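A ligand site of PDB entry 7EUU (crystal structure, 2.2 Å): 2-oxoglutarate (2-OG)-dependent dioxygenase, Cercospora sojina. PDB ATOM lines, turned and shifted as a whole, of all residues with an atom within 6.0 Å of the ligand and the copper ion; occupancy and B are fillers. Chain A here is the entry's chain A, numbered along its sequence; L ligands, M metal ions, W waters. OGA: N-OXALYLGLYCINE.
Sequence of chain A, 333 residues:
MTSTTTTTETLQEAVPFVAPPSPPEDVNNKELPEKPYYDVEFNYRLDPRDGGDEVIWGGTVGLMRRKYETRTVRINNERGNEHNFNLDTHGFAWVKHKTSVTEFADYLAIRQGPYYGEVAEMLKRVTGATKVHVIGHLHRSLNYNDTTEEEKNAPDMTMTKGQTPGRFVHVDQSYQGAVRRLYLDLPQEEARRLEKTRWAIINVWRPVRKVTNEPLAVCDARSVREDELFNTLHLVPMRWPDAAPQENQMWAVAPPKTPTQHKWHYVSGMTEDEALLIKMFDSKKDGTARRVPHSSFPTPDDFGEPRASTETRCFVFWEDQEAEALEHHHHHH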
ATOM      1  N   ARG A 140     -10.429  15.629 -24.715  1.00  0.00           N
ATOM      2  CA  ARG A 140     -10.674  15.314 -23.279  1.00  0.00           C
ATOM      3  C   ARG A 140     -11.851  14.335 -23.200  1.00  0.00           C
ATOM      4  O   ARG A 140     -12.897  14.621 -23.822  1.00  0.00           O
ATOM      5  CB  ARG A 140     -10.956  16.591 -22.494  1.00  0.00           C
ATOM      6  CG  ARG A 140     -10.228  17.820 -23.019  1.00  0.00           C
ATOM      7  CD  ARG A 140     -10.264  18.979 -22.040  1.00  0.00           C
ATOM      8  NE  ARG A 140      -9.276  18.850 -20.982  1.00  0.00           N
ATOM      9  CZ  ARG A 140      -8.464  19.830 -20.593  1.00  0.00           C
ATOM     10  NH1 ARG A 140      -8.532  21.009 -21.164  1.00  0.00           N
ATOM     11  NH2 ARG A 140      -7.589  19.607 -19.616  1.00  0.00           N
ATOM     12  N   THR A 164      -8.242  14.374 -18.541  1.00  0.00           N
ATOM     13  CA  THR A 164      -9.287  14.735 -17.603  1.00  0.00           C
ATOM     14  C   THR A 164      -9.733  16.170 -17.900  1.00  0.00           C
ATOM     15  O   THR A 164      -9.076  16.891 -18.651  1.00  0.00           O
ATOM     16  CB  THR A 164      -8.752  14.582 -16.184  1.00  0.00           C
ATOM     17  OG1 THR A 164      -9.823  14.321 -15.269  1.00  0.00           O
ATOM     18  CG2 THR A 164      -8.005  15.822 -15.753  1.00  0.00           C
ATOM     19  N   PRO A 165     -10.875  16.613 -17.361  1.00  0.00           N
ATOM     20  CA  PRO A 165     -11.275  18.012 -17.563  1.00  0.00           C
ATOM     21  C   PRO A 165     -10.294  18.975 -16.910  1.00  0.00           C
ATOM     22  O   PRO A 165      -9.533  18.627 -16.009  1.00  0.00           O
ATOM     23  CB  PRO A 165     -12.654  18.095 -16.908  1.00  0.00           C
ATOM     24  CG  PRO A 165     -13.143  16.693 -16.876  1.00  0.00           C
ATOM     25  CD  PRO A 165     -11.936  15.834 -16.705  1.00  0.00           C
ATOM     26  N   GLY A 166     -10.314  20.212 -17.397  1.00  0.00           N
ATOM     27  CA  GLY A 166      -9.420  21.234 -16.887  1.00  0.00           C
ATOM     28  C   GLY A 166      -9.990  21.979 -15.693  1.00  0.00           C
ATOM     29  O   GLY A 166     -10.560  23.058 -15.846  1.00  0.00           O
ATOM     30  N   ARG A 167      -9.844  21.399 -14.501  1.00  0.00           N
ATOM     31  CA  ARG A 167     -10.495  21.919 -13.310  1.00  0.00           C
ATOM     32  C   ARG A 167      -9.535  22.829 -12.536  1.00  0.00           C
ATOM     33  O   ARG A 167      -9.085  22.510 -11.422  1.00  0.00           O
ATOM     34  CB  ARG A 167     -11.014  20.771 -12.449  1.00  0.00           C
ATOM     35  CG  ARG A 167     -12.277  21.111 -11.685  1.00  0.00           C
ATOM     36  CD  ARG A 167     -12.677  19.997 -10.742  1.00  0.00           C
ATOM     37  NE  ARG A 167     -13.563  19.024 -11.376  1.00  0.00           N
ATOM     38  CZ  ARG A 167     -14.068  17.957 -10.771  1.00  0.00           C
ATOM     39  NH1 ARG A 167     -13.762  17.718  -9.498  1.00  0.00           N
ATOM     40  NH2 ARG A 167     -14.859  17.131 -11.430  1.00  0.00           N
ATOM     41  N   HIS A 170      -7.594  29.319 -15.397  1.00  0.00           N
ATOM     42  CA  HIS A 170      -6.384  29.593 -16.142  1.00  0.00           C
ATOM     43  C   HIS A 170      -6.734  30.305 -17.436  1.00  0.00           C
ATOM     44  O   HIS A 170      -7.890  30.308 -17.883  1.00  0.00           O
ATOM     45  CB  HIS A 170      -5.622  28.307 -16.455  1.00  0.00           C
ATOM     46  CG  HIS A 170      -6.296  27.427 -17.468  1.00  0.00           C
ATOM     47  ND1 HIS A 170      -7.271  26.511 -17.121  1.00  0.00           N
ATOM     48  CD2 HIS A 170      -6.160  27.340 -18.804  1.00  0.00           C
ATOM     49  CE1 HIS A 170      -7.693  25.900 -18.212  1.00  0.00           C
ATOM     50  NE2 HIS A 170      -7.041  26.378 -19.243  1.00  0.00           N
ATOM     51  N   VAL A 171      -5.721  30.926 -18.027  1.00  0.00           N
ATOM     52  CA  VAL A 171      -5.734  31.322 -19.432  1.00  0.00           C
ATOM     53  C   VAL A 171      -4.617  30.532 -20.113  1.00  0.00           C
ATOM     54  O   VAL A 171      -3.512  30.429 -19.567  1.00  0.00           O
ATOM     55  CB  VAL A 171      -5.528  32.841 -19.607  1.00  0.00           C
ATOM     56  CG1 VAL A 171      -5.824  33.245 -21.043  1.00  0.00           C
ATOM     57  CG2 VAL A 171      -6.419  33.606 -18.641  1.00  0.00           C
ATOM     58  N   ASP A 172      -4.914  29.974 -21.276  1.00  0.00           N
ATOM     59  CA  ASP A 172      -3.977  29.047 -21.921  1.00  0.00           C
ATOM     60  C   ASP A 172      -2.650  29.706 -22.273  1.00  0.00           C
ATOM     61  O   ASP A 172      -1.645  29.002 -22.395  1.00  0.00           O
ATOM     62  CB  ASP A 172      -4.611  28.447 -23.169  1.00  0.00           C
ATOM     63  CG  ASP A 172      -5.599  27.344 -22.854  1.00  0.00           C
ATOM     64  OD1 ASP A 172      -6.363  27.501 -21.875  1.00  0.00           O
ATOM     65  OD2 ASP A 172      -5.613  26.334 -23.575  1.00  0.00           O
ATOM     66  N   ASN A 203      -9.365  29.694 -28.553  1.00  0.00           N
ATOM     67  CA  ASN A 203      -9.639  28.267 -28.451  1.00  0.00           C
ATOM     68  C   ASN A 203     -11.086  28.004 -28.854  1.00  0.00           C
ATOM     69  O   ASN A 203     -11.995  28.746 -28.458  1.00  0.00           O
ATOM     70  CB  ASN A 203      -9.394  27.749 -27.040  1.00  0.00           C
ATOM     71  CG  ASN A 203      -7.966  27.278 -26.827  1.00  0.00           C
ATOM     72  OD1 ASN A 203      -7.063  27.675 -27.559  1.00  0.00           O
ATOM     73  ND2 ASN A 203      -7.758  26.446 -25.813  1.00  0.00           N
ATOM     74  N   TRP A 205     -13.859  25.359 -28.448  1.00  0.00           N
ATOM     75  CA  TRP A 205     -14.212  24.230 -27.600  1.00  0.00           C
ATOM     76  C   TRP A 205     -15.548  23.647 -28.073  1.00  0.00           C
ATOM     77  O   TRP A 205     -16.546  24.366 -28.156  1.00  0.00           O
ATOM     78  CB  TRP A 205     -14.313  24.699 -26.146  1.00  0.00           C
ATOM     79  CG  TRP A 205     -14.485  23.603 -25.135  1.00  0.00           C
ATOM     80  CD1 TRP A 205     -13.498  22.950 -24.453  1.00  0.00           C
ATOM     81  CD2 TRP A 205     -15.729  23.049 -24.669  1.00  0.00           C
ATOM     82  NE1 TRP A 205     -14.043  22.023 -23.598  1.00  0.00           N
ATOM     83  CE2 TRP A 205     -15.411  22.061 -23.719  1.00  0.00           C
ATOM     84  CE3 TRP A 205     -17.063  23.290 -24.976  1.00  0.00           C
ATOM     85  CZ2 TRP A 205     -16.391  21.311 -23.064  1.00  0.00           C
ATOM     86  CZ3 TRP A 205     -18.035  22.543 -24.327  1.00  0.00           C
ATOM     87  CH2 TRP A 205     -17.697  21.569 -23.380  1.00  0.00           C
ATOM     88  N   GLU A 214     -19.776  18.044 -16.121  1.00  0.00           N
ATOM     89  CA  GLU A 214     -18.543  18.818 -16.167  1.00  0.00           C
ATOM     90  C   GLU A 214     -18.493  19.792 -17.349  1.00  0.00           C
ATOM     91  O   GLU A 214     -17.662  19.647 -18.254  1.00  0.00           O
ATOM     92  CB  GLU A 214     -17.317  17.901 -16.179  1.00  0.00           C
ATOM     93  CG  GLU A 214     -16.013  18.606 -15.821  1.00  0.00           C
ATOM     94  CD  GLU A 214     -15.543  18.295 -14.411  1.00  0.00           C
ATOM     95  OE1 GLU A 214     -15.907  17.233 -13.873  1.00  0.00           O
ATOM     96  OE2 GLU A 214     -14.788  19.118 -13.851  1.00  0.00           O
ATOM     97  N   PRO A 215     -19.374  20.801 -17.377  1.00  0.00           N
ATOM     98  CA  PRO A 215     -19.325  21.800 -18.449  1.00  0.00           C
ATOM     99  C   PRO A 215     -18.129  22.739 -18.300  1.00  0.00           C
ATOM    100  O   PRO A 215     -17.362  22.616 -17.342  1.00  0.00           O
ATOM    101  CB  PRO A 215     -20.649  22.543 -18.309  1.00  0.00           C
ATOM    102  CG  PRO A 215     -20.964  22.437 -16.856  1.00  0.00           C
ATOM    103  CD  PRO A 215     -20.464  21.089 -16.422  1.00  0.00           C
ATOM    104  N   LEU A 216     -17.977  23.672 -19.228  1.00  0.00           N
ATOM    105  CA  LEU A 216     -16.867  24.610 -19.240  1.00  0.00           C
ATOM    106  C   LEU A 216     -17.375  26.017 -18.940  1.00  0.00           C
ATOM    107  O   LEU A 216     -18.298  26.498 -19.600  1.00  0.00           O
ATOM    108  CB  LEU A 216     -16.136  24.591 -20.584  1.00  0.00           C
ATOM    109  CG  LEU A 216     -14.827  25.374 -20.663  1.00  0.00           C
ATOM    110  CD1 LEU A 216     -13.833  24.847 -19.639  1.00  0.00           C
ATOM    111  CD2 LEU A 216     -14.256  25.279 -22.056  1.00  0.00           C
ATOM    112  N   MET A 250       1.256  30.049 -19.187  1.00  0.00           N
ATOM    113  CA  MET A 250      -0.145  30.335 -18.926  1.00  0.00           C
ATOM    114  C   MET A 250      -0.292  31.521 -17.981  1.00  0.00           C
ATOM    115  O   MET A 250       0.672  31.999 -17.374  1.00  0.00           O
ATOM    116  CB  MET A 250      -0.837  29.109 -18.304  1.00  0.00           C
ATOM    117  CG  MET A 250      -1.085  27.942 -19.235  1.00  0.00           C
ATOM    118  SD  MET A 250      -2.141  26.714 -18.432  1.00  0.00           S
ATOM    119  CE  MET A 250      -2.885  25.902 -19.849  1.00  0.00           C
ATOM    120  N   ILE A 278     -13.087  30.897 -27.016  1.00  0.00           N
ATOM    121  CA  ILE A 278     -12.479  31.453 -25.819  1.00  0.00           C
ATOM    122  C   ILE A 278     -11.214  32.194 -26.222  1.00  0.00           C
ATOM    123  O   ILE A 278     -10.282  31.589 -26.775  1.00  0.00           O
ATOM    124  CB  ILE A 278     -12.167  30.366 -24.778  1.00  0.00           C
ATOM    125  CG1 ILE A 278     -13.396  29.499 -24.525  1.00  0.00           C
ATOM    126  CG2 ILE A 278     -11.671  30.993 -23.482  1.00  0.00           C
ATOM    127  CD1 ILE A 278     -13.130  28.288 -23.673  1.00  0.00           C
ATOM    128  N   MET A 280      -7.806  33.663 -25.602  1.00  0.00           N
ATOM    129  CA  MET A 280      -6.667  33.588 -24.698  1.00  0.00           C
ATOM    130  C   MET A 280      -5.789  34.827 -24.786  1.00  0.00           C
ATOM    131  O   MET A 280      -5.247  35.275 -23.765  1.00  0.00           O
ATOM    132  CB  MET A 280      -5.823  32.353 -25.003  1.00  0.00           C
ATOM    133  CG  MET A 280      -6.622  31.059 -25.067  1.00  0.00           C
ATOM    134  SD  MET A 280      -7.584  30.800 -23.571  1.00  0.00           S
ATOM    135  CE  MET A 280      -8.471  29.313 -24.021  1.00  0.00           C
ATOM    136  N   HIS A 294     -10.772  30.662 -17.477  1.00  0.00           N
ATOM    137  CA  HIS A 294     -11.783  29.648 -17.715  1.00  0.00           C
ATOM    138  C   HIS A 294     -11.408  28.394 -16.939  1.00  0.00           C
ATOM    139  O   HIS A 294     -10.266  28.215 -16.523  1.00  0.00           O
ATOM    140  CB  HIS A 294     -11.939  29.337 -19.210  1.00  0.00           C
ATOM    141  CG  HIS A 294     -10.676  28.846 -19.845  1.00  0.00           C
ATOM    142  ND1 HIS A 294      -9.633  29.685 -20.183  1.00  0.00           N
ATOM    143  CD2 HIS A 294     -10.283  27.601 -20.204  1.00  0.00           C
ATOM    144  CE1 HIS A 294      -8.659  28.976 -20.718  1.00  0.00           C
ATOM    145  NE2 HIS A 294      -9.023  27.709 -20.742  1.00  0.00           N
ATOM    146  N   SER A 295     -12.410  27.532 -16.741  1.00  0.00           N
ATOM    147  CA  SER A 295     -12.232  26.316 -15.973  1.00  0.00           C
ATOM    148  C   SER A 295     -13.473  25.460 -16.135  1.00  0.00           C
ATOM    149  O   SER A 295     -14.583  25.987 -16.215  1.00  0.00           O
ATOM    150  CB  SER A 295     -12.002  26.623 -14.482  1.00  0.00           C
ATOM    151  OG  SER A 295     -11.957  25.437 -13.708  1.00  0.00           O
ATOM    152  N   SER A 296     -13.269  24.144 -16.210  1.00  0.00           N
ATOM    153  CA  SER A 296     -14.408  23.254 -16.083  1.00  0.00           C
ATOM    154  C   SER A 296     -14.853  23.200 -14.629  1.00  0.00           C
ATOM    155  O   SER A 296     -14.146  23.641 -13.715  1.00  0.00           O
ATOM    156  CB  SER A 296     -14.052  21.854 -16.596  1.00  0.00           C
ATOM    157  OG  SER A 296     -13.206  21.187 -15.683  1.00  0.00           O
ATOM    158  N   ARG A 307     -18.206  13.557 -19.890  1.00  0.00           N
ATOM    159  CA  ARG A 307     -18.151  14.576 -20.931  1.00  0.00           C
ATOM    160  C   ARG A 307     -16.905  14.401 -21.776  1.00  0.00           C
ATOM    161  O   ARG A 307     -15.822  14.120 -21.256  1.00  0.00           O
ATOM    162  CB  ARG A 307     -18.186  15.971 -20.304  1.00  0.00           C
ATOM    163  CG  ARG A 307     -18.139  17.130 -21.305  1.00  0.00           C
ATOM    164  CD  ARG A 307     -16.722  17.695 -21.438  1.00  0.00           C
ATOM    165  NE  ARG A 307     -16.371  18.565 -20.312  1.00  0.00           N
ATOM    166  CZ  ARG A 307     -15.201  19.181 -20.194  1.00  0.00           C
ATOM    167  NH1 ARG A 307     -14.255  19.023 -21.121  1.00  0.00           N
ATOM    168  NH2 ARG A 307     -14.956  19.949 -19.141  1.00  0.00           N
ATOM    169  N   SER A 309     -14.756  16.191 -25.227  1.00  0.00           N
ATOM    170  CA  SER A 309     -14.666  17.438 -25.971  1.00  0.00           C
ATOM    171  C   SER A 309     -13.317  17.514 -26.658  1.00  0.00           C
ATOM    172  O   SER A 309     -12.382  16.778 -26.327  1.00  0.00           O
ATOM    173  CB  SER A 309     -14.857  18.647 -25.058  1.00  0.00           C
ATOM    174  OG  SER A 309     -13.881  18.650 -24.019  1.00  0.00           O
ATOM    175  N   GLU A 311     -10.676  20.869 -27.770  1.00  0.00           N
ATOM    176  CA  GLU A 311     -10.382  22.286 -27.799  1.00  0.00           C
ATOM    177  C   GLU A 311      -9.305  22.516 -28.852  1.00  0.00           C
ATOM    178  O   GLU A 311      -8.223  21.940 -28.759  1.00  0.00           O
ATOM    179  CB  GLU A 311      -9.937  22.795 -26.427  1.00  0.00           C
ATOM    180  CG  GLU A 311      -8.791  22.028 -25.798  1.00  0.00           C
ATOM    181  CD  GLU A 311      -8.901  21.946 -24.288  1.00  0.00           C
ATOM    182  OE1 GLU A 311      -9.965  21.515 -23.794  1.00  0.00           O
ATOM    183  OE2 GLU A 311      -7.923  22.310 -23.602  1.00  0.00           O
ATOM    184  N   ARG A 313      -6.830  24.964 -30.612  1.00  0.00           N
ATOM    185  CA  ARG A 313      -6.025  26.202 -30.459  1.00  0.00           C
ATOM    186  C   ARG A 313      -5.879  26.850 -31.836  1.00  0.00           C
ATOM    187  O   ARG A 313      -5.500  26.140 -32.794  1.00  0.00           O
ATOM    188  CB  ARG A 313      -4.658  25.869 -29.855  1.00  0.00           C
ATOM    189  CG  ARG A 313      -4.687  24.764 -28.812  1.00  0.00           C
ATOM    190  CD  ARG A 313      -3.846  25.085 -27.597  1.00  0.00           C
ATOM    191  NE  ARG A 313      -4.624  25.069 -26.363  1.00  0.00           N
ATOM    192  CZ  ARG A 313      -4.885  23.980 -25.649  1.00  0.00           C
ATOM    193  NH1 ARG A 313      -4.427  22.804 -26.051  1.00  0.00           N
ATOM    194  NH2 ARG A 313      -5.601  24.068 -24.548  1.00  0.00           N
HETATM  195  C1  OGA L   1      -9.628  24.885 -22.892  1.00  0.00           C
HETATM  196  C2  OGA L   1      -9.929  24.303 -21.509  1.00  0.00           C
HETATM  197  C4  OGA L   1     -10.960  22.490 -20.110  1.00  0.00           C
HETATM  198  C5  OGA L   1     -11.989  21.375 -20.274  1.00  0.00           C
HETATM  199  O1  OGA L   1     -10.357  24.586 -23.868  1.00  0.00           O
HETATM  200  O2  OGA L   1      -8.645  25.668 -23.043  1.00  0.00           O
HETATM  201  O2' OGA L   1      -9.550  24.860 -20.542  1.00  0.00           O
HETATM  202  O3  OGA L   1     -12.273  20.635 -19.296  1.00  0.00           O
HETATM  203  N1  OGA L   1     -10.668  23.055 -21.410  1.00  0.00           N
HETATM  204  O4  OGA L   1     -12.540  21.198 -21.394  1.00  0.00           O
HETATM  205 CU    CU M   1      -7.832  26.159 -21.129  1.00  0.00          CU
HETATM  206  O   HOH W   1      -6.408  24.462 -21.620  1.00  0.00           O
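N of Gly 166 sits at hydrogen-bond distance from O3 of the ligand (2.8 Å).
The guanidinium group of Arg 307 is in salt-bridge range of an oxygen (O3) of the ligand, at 2.8 Å.
The indole nitrogen (NE1) of Trp 205 lies within hydrogen-bond range of an oxygen (O4) of the ligand (2.8 Å).
N1 of the ligand sits at hydrogen-bond distance from OE1 of Glu 311, at 2.9 Å.
The guanidinium group (NE) of Arg 140 is in salt-bridge range of an oxygen (O3) of the ligand (3.9 Å).
The side-chain amide nitrogen of Asn 203 sits close to an oxygen (O2) of the ligand (3.0 Å).
The guanidinium group (NH2) of Arg 313 sits close to an oxygen (O2) of the ligand.
Residues that only touch the ligand: Pro 165 (3.3 Å), Leu 216 (3.7 Å), Met 280 (3.8 Å), Ser 296 (3.5 Å) and Ser 309 (3.9 Å).
Hydrophobic or aromatic side chains within 4 Å of the ligand: Pro 165, His 170, Trp 205, Leu 216, Met 280 and His 294.
Of the 23 residues printed, 15 come within 4 Å of the ligand.
OD2 of Asp 172 is in salt-bridge range of NH2 of Arg 313, 2.5 Å away.
The backbone NH (N) of Asp 172 is in hydrogen-bond range of the side-chain sulfur (SD) of Met 280 (3.6 Å).
OG of Ser 295 sits at hydrogen-bond distance from O of Gly 166 (3.5 Å).
The guanidinium group of Arg 307 lies within hydrogen-bond range of the side-chain hydroxyl of Ser 309 (2.9 Å).
OE2 of Glu 311 lies within salt-bridge range of NH1 of Arg 140, 2.8 Å away.
NH2 of Arg 313 sits close to ND2 of Asn 203 (3.5 Å).
N of Asn 203 lies within hydrogen-bond range of O of Ile 278, at 2.8 Å.
The side-chain hydroxyl (OG) of Ser 296 sits at hydrogen-bond distance from the side-chain carboxylate (OE2) of Glu 214 (3.2 Å).
Water W1 lies within hydrogen-bond range of OD2 of Asp 172 (2.8 Å), NH2 of Arg 313 (3.1 Å) and OE2 of Glu 311 (3.3 Å).
Within 4 Å of the copper ion: His 170, Asp 172 and His 294.
Along chain A the residues within 4 Å of the copper ion span positions 170 to 294.
The nearest printed residue that does not touch the copper ion is Met 280 (4.3 Å).
The copper ion is bound by NE2 of His 294 (2.0 Å).
The copper ion is bound by NE2 of His 170.
OD1 of Asp 172 is bound to the copper ion (2.1 Å).
O2 of the ligand binds the copper ion.
An oxygen (O2') of the ligand binds the copper ion (2.2 Å).
Water W1 is bound to the copper ion, at 2.3 Å.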
